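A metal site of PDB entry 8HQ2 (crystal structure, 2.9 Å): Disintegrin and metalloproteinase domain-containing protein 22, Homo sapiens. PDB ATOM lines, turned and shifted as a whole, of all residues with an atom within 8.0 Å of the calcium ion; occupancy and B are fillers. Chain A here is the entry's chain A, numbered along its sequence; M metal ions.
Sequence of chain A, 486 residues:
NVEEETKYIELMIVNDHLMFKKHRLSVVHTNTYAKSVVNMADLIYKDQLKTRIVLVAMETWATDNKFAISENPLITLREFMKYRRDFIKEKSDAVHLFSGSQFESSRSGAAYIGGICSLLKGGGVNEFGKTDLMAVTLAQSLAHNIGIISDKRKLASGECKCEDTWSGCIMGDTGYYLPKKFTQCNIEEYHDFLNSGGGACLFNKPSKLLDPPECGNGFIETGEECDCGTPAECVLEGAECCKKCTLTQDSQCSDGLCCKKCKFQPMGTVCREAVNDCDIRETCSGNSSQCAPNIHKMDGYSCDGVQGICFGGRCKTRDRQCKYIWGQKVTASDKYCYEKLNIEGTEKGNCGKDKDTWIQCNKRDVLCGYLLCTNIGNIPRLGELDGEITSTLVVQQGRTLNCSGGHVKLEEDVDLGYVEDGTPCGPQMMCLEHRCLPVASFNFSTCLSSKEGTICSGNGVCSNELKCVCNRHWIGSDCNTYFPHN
The side-chain carboxylate (OD2) of Asp 227 sits close to the backbone NH (N) of Gly 216 (3.2 Å). OD1 of Asp 227 is in hydrogen-bond range of N of Gly 218 (2.9 Å). OD1 of Asp 227 sits at hydrogen-bond distance from N of Gly 229. The backbone NH (N) of Glu 221 sits close to the side-chain carboxylate (OE1) of Glu 224 (2.8 Å). ND2 of Asn 217 sits at hydrogen-bond distance from OE1 of Glu 221, 3.1 Å away. The side-chain sulfur of Cys 245 forms a disulfide with the side-chain sulfur of Cys 215.
Within 4 Å of the calcium ion: Glu 214, Asn 217, Phe 219, Glu 221, Glu 224 and Asp 227. The nearest printed residue that does not touch the calcium ion is Cys 215 (4.2 Å).
The calcium ion is bound by the side-chain carboxylate (OD2) of Asp 227, the side-chain carboxylate (OE1) of Glu 224, the side-chain amide oxygen (OD1) of Asn 217, the side-chain carboxylate (OE2) of Glu 224, the backbone carbonyl oxygen (O) of Phe 219 and the backbone carbonyl oxygen (O) of Glu 214. The calcium ion has six donor atoms within binding distance. Slightly farther from the calcium ion lies OE2 of Glu 221 (3.0 Å).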
ATOM      1  N   SER A 207      -7.793  24.284  18.364  1.00  0.00           N
ATOM      2  CA  SER A 207      -8.772  24.372  19.438  1.00  0.00           C
ATOM      3  C   SER A 207     -10.196  24.140  18.939  1.00  0.00           C
ATOM      4  O   SER A 207     -10.988  23.450  19.591  1.00  0.00           O
ATOM      5  CB  SER A 207      -8.666  25.726  20.140  1.00  0.00           C
ATOM      6  OG  SER A 207      -8.718  26.795  19.206  1.00  0.00           O
ATOM      7  N   LEU A 209     -12.898  23.280  15.539  1.00  0.00           N
ATOM      8  CA  LEU A 209     -12.995  22.613  14.244  1.00  0.00           C
ATOM      9  C   LEU A 209     -14.367  22.891  13.639  1.00  0.00           C
ATOM     10  O   LEU A 209     -15.342  23.168  14.344  1.00  0.00           O
ATOM     11  CB  LEU A 209     -12.769  21.095  14.367  1.00  0.00           C
ATOM     12  CG  LEU A 209     -11.417  20.576  14.893  1.00  0.00           C
ATOM     13  CD1 LEU A 209     -11.269  20.743  16.400  1.00  0.00           C
ATOM     14  CD2 LEU A 209     -11.247  19.119  14.511  1.00  0.00           C
ATOM     15  N   PRO A 212     -19.071  19.359  13.779  1.00  0.00           N
ATOM     16  CA  PRO A 212     -19.599  19.381  15.143  1.00  0.00           C
ATOM     17  C   PRO A 212     -18.709  18.576  16.073  1.00  0.00           C
ATOM     18  O   PRO A 212     -18.190  17.510  15.694  1.00  0.00           O
ATOM     19  CB  PRO A 212     -20.982  18.733  14.999  1.00  0.00           C
ATOM     20  CG  PRO A 212     -20.944  18.018  13.684  1.00  0.00           C
ATOM     21  CD  PRO A 212     -20.056  18.840  12.816  1.00  0.00           C
ATOM     22  N   PRO A 213     -18.491  19.061  17.298  1.00  0.00           N
ATOM     23  CA  PRO A 213     -17.548  18.382  18.196  1.00  0.00           C
ATOM     24  C   PRO A 213     -17.987  16.961  18.526  1.00  0.00           C
ATOM     25  O   PRO A 213     -19.154  16.717  18.822  1.00  0.00           O
ATOM     26  CB  PRO A 213     -17.548  19.277  19.444  1.00  0.00           C
ATOM     27  CG  PRO A 213     -18.823  20.069  19.353  1.00  0.00           C
ATOM     28  CD  PRO A 213     -19.067  20.266  17.889  1.00  0.00           C
ATOM     29  N   GLU A 214     -17.035  16.043  18.459  1.00  0.00           N
ATOM     30  CA  GLU A 214     -17.232  14.662  18.867  1.00  0.00           C
ATOM     31  C   GLU A 214     -16.188  14.310  19.913  1.00  0.00           C
ATOM     32  O   GLU A 214     -15.037  14.780  19.849  1.00  0.00           O
ATOM     33  CB  GLU A 214     -17.136  13.695  17.672  1.00  0.00           C
ATOM     34  CG  GLU A 214     -15.721  13.411  17.191  1.00  0.00           C
ATOM     35  CD  GLU A 214     -15.665  12.419  16.039  1.00  0.00           C
ATOM     36  OE1 GLU A 214     -16.086  11.257  16.246  1.00  0.00           O
ATOM     37  OE2 GLU A 214     -15.197  12.795  14.945  1.00  0.00           O
ATOM     38  N   CYS A 215     -16.576  13.507  20.891  1.00  0.00           N
ATOM     39  CA  CYS A 215     -15.638  13.087  21.927  1.00  0.00           C
ATOM     40  C   CYS A 215     -14.784  11.931  21.422  1.00  0.00           C
ATOM     41  O   CYS A 215     -15.258  11.045  20.713  1.00  0.00           O
ATOM     42  CB  CYS A 215     -16.368  12.679  23.195  1.00  0.00           C
ATOM     43  SG  CYS A 215     -15.214  12.165  24.482  1.00  0.00           S
ATOM     44  N   GLY A 216     -13.516  11.953  21.815  1.00  0.00           N
ATOM     45  CA  GLY A 216     -12.588  10.909  21.439  1.00  0.00           C
ATOM     46  C   GLY A 216     -11.870  11.100  20.129  1.00  0.00           C
ATOM     47  O   GLY A 216     -11.238  10.148  19.646  1.00  0.00           O
ATOM     48  N   ASN A 217     -11.940  12.282  19.518  1.00  0.00           N
ATOM     49  CA  ASN A 217     -11.264  12.549  18.264  1.00  0.00           C
ATOM     50  C   ASN A 217      -9.834  13.017  18.451  1.00  0.00           C
ATOM     51  O   ASN A 217      -9.103  13.151  17.458  1.00  0.00           O
ATOM     52  CB  ASN A 217     -12.040  13.578  17.441  1.00  0.00           C
ATOM     53  CG  ASN A 217     -12.140  14.920  18.132  1.00  0.00           C
ATOM     54  OD1 ASN A 217     -12.044  15.006  19.356  1.00  0.00           O
ATOM     55  ND2 ASN A 217     -12.321  15.979  17.354  1.00  0.00           N
ATOM     56  N   GLY A 218      -9.401  13.266  19.689  1.00  0.00           N
ATOM     57  CA  GLY A 218      -8.052  13.699  19.973  1.00  0.00           C
ATOM     58  C   GLY A 218      -7.838  15.192  20.036  1.00  0.00           C
ATOM     59  O   GLY A 218      -6.760  15.637  20.449  1.00  0.00           O
ATOM     60  N   PHE A 219      -8.841  15.994  19.673  1.00  0.00           N
ATOM     61  CA  PHE A 219      -8.762  17.449  19.735  1.00  0.00           C
ATOM     62  C   PHE A 219      -9.793  17.955  20.724  1.00  0.00           C
ATOM     63  O   PHE A 219     -10.972  17.579  20.650  1.00  0.00           O
ATOM     64  CB  PHE A 219      -9.002  18.071  18.354  1.00  0.00           C
ATOM     65  CG  PHE A 219      -8.038  17.622  17.302  1.00  0.00           C
ATOM     66  CD1 PHE A 219      -6.671  17.667  17.528  1.00  0.00           C
ATOM     67  CD2 PHE A 219      -8.502  17.140  16.086  1.00  0.00           C
ATOM     68  CE1 PHE A 219      -5.789  17.252  16.557  1.00  0.00           C
ATOM     69  CE2 PHE A 219      -7.614  16.718  15.105  1.00  0.00           C
ATOM     70  CZ  PHE A 219      -6.247  16.777  15.340  1.00  0.00           C
ATOM     71  N   ILE A 220      -9.358  18.795  21.660  1.00  0.00           N
ATOM     72  CA  ILE A 220     -10.301  19.404  22.587  1.00  0.00           C
ATOM     73  C   ILE A 220     -11.167  20.402  21.830  1.00  0.00           C
ATOM     74  O   ILE A 220     -10.718  21.067  20.881  1.00  0.00           O
ATOM     75  CB  ILE A 220      -9.565  20.066  23.777  1.00  0.00           C
ATOM     76  CG1 ILE A 220      -9.362  21.562  23.550  1.00  0.00           C
ATOM     77  CG2 ILE A 220      -8.235  19.367  24.029  1.00  0.00           C
ATOM     78  CD1 ILE A 220     -10.300  22.445  24.363  1.00  0.00           C
ATOM     79  N   GLU A 221     -12.440  20.441  22.226  1.00  0.00           N
ATOM     80  CA  GLU A 221     -13.448  21.340  21.593  1.00  0.00           C
ATOM     81  C   GLU A 221     -14.243  22.039  22.707  1.00  0.00           C
ATOM     82  O   GLU A 221     -14.234  21.526  23.846  1.00  0.00           O
ATOM     83  CB  GLU A 221     -14.371  20.555  20.661  1.00  0.00           C
ATOM     84  CG  GLU A 221     -13.837  20.436  19.245  1.00  0.00           C
ATOM     85  CD  GLU A 221     -13.866  19.037  18.664  1.00  0.00           C
ATOM     86  OE1 GLU A 221     -13.441  18.860  17.508  1.00  0.00           O
ATOM     87  OE2 GLU A 221     -14.327  18.117  19.374  1.00  0.00           O
ATOM     88  N   THR A 222     -14.859  23.173  22.411  1.00  0.00           N
ATOM     89  CA  THR A 222     -15.603  23.919  23.409  1.00  0.00           C
ATOM     90  C   THR A 222     -16.610  22.996  24.109  1.00  0.00           C
ATOM     91  O   THR A 222     -17.309  22.210  23.460  1.00  0.00           O
ATOM     92  CB  THR A 222     -16.304  25.124  22.789  1.00  0.00           C
ATOM     93  OG1 THR A 222     -17.054  25.821  23.791  1.00  0.00           O
ATOM     94  CG2 THR A 222     -17.233  24.696  21.645  1.00  0.00           C
ATOM     95  N   GLU A 224     -15.595  20.577  25.978  1.00  0.00           N
ATOM     96  CA  GLU A 224     -14.815  19.381  26.273  1.00  0.00           C
ATOM     97  C   GLU A 224     -13.720  19.728  27.267  1.00  0.00           C
ATOM     98  O   GLU A 224     -12.824  20.527  26.953  1.00  0.00           O
ATOM     99  CB  GLU A 224     -14.211  18.780  25.007  1.00  0.00           C
ATOM    100  CG  GLU A 224     -15.175  18.040  24.123  1.00  0.00           C
ATOM    101  CD  GLU A 224     -14.492  17.479  22.900  1.00  0.00           C
ATOM    102  OE1 GLU A 224     -13.333  17.863  22.653  1.00  0.00           O
ATOM    103  OE2 GLU A 224     -15.101  16.642  22.202  1.00  0.00           O
ATOM    104  N   GLU A 225     -13.799  19.156  28.475  1.00  0.00           N
ATOM    105  CA  GLU A 225     -12.745  19.359  29.452  1.00  0.00           C
ATOM    106  C   GLU A 225     -11.417  18.768  28.981  1.00  0.00           C
ATOM    107  O   GLU A 225     -10.355  19.347  29.213  1.00  0.00           O
ATOM    108  CB  GLU A 225     -13.165  18.756  30.796  1.00  0.00           C
ATOM    109  CG  GLU A 225     -14.203  19.575  31.547  1.00  0.00           C
ATOM    110  CD  GLU A 225     -14.848  18.801  32.673  1.00  0.00           C
ATOM    111  OE1 GLU A 225     -14.657  17.576  32.741  1.00  0.00           O
ATOM    112  OE2 GLU A 225     -15.554  19.420  33.499  1.00  0.00           O
ATOM    113  N   CYS A 226     -11.475  17.623  28.309  1.00  0.00           N
ATOM    114  CA  CYS A 226     -10.266  16.952  27.840  1.00  0.00           C
ATOM    115  C   CYS A 226     -10.628  16.017  26.699  1.00  0.00           C
ATOM    116  O   CYS A 226     -11.782  15.620  26.535  1.00  0.00           O
ATOM    117  CB  CYS A 226      -9.601  16.182  28.976  1.00  0.00           C
ATOM    118  SG  CYS A 226     -10.703  15.068  29.887  1.00  0.00           S
ATOM    119  N   ASP A 227      -9.621  15.683  25.896  1.00  0.00           N
ATOM    120  CA  ASP A 227      -9.772  14.641  24.877  1.00  0.00           C
ATOM    121  C   ASP A 227      -8.501  13.795  24.832  1.00  0.00           C
ATOM    122  O   ASP A 227      -7.431  14.314  24.526  1.00  0.00           O
ATOM    123  CB  ASP A 227     -10.054  15.250  23.509  1.00  0.00           C
ATOM    124  CG  ASP A 227     -10.741  14.277  22.575  1.00  0.00           C
ATOM    125  OD1 ASP A 227     -10.234  13.138  22.423  1.00  0.00           O
ATOM    126  OD2 ASP A 227     -11.788  14.634  22.000  1.00  0.00           O
ATOM    127  N   CYS A 228      -8.633  12.505  25.130  1.00  0.00           N
ATOM    128  CA  CYS A 228      -7.505  11.581  25.037  1.00  0.00           C
ATOM    129  C   CYS A 228      -7.465  10.796  23.737  1.00  0.00           C
ATOM    130  O   CYS A 228      -6.501  10.055  23.504  1.00  0.00           O
ATOM    131  CB  CYS A 228      -7.529  10.603  26.217  1.00  0.00           C
ATOM    132  SG  CYS A 228      -8.892   9.418  26.190  1.00  0.00           S
ATOM    133  N   GLY A 229      -8.478  10.930  22.870  1.00  0.00           N
ATOM    134  CA  GLY A 229      -8.501  10.211  21.617  1.00  0.00           C
ATOM    135  C   GLY A 229      -9.108   8.821  21.669  1.00  0.00           C
ATOM    136  O   GLY A 229      -9.970   8.543  22.509  1.00  0.00           O
ATOM    137  N   CYS A 245     -14.409  12.487  27.648  1.00  0.00           N
ATOM    138  CA  CYS A 245     -14.144  13.925  27.564  1.00  0.00           C
ATOM    139  C   CYS A 245     -14.581  14.671  28.821  1.00  0.00           C
ATOM    140  O   CYS A 245     -14.990  15.829  28.757  1.00  0.00           O
ATOM    141  CB  CYS A 245     -14.782  14.531  26.320  1.00  0.00           C
ATOM    142  SG  CYS A 245     -14.116  13.838  24.798  1.00  0.00           S
HETATM  143 CA    CA M   1     -12.933  16.188  21.166  1.00  0.00          CA
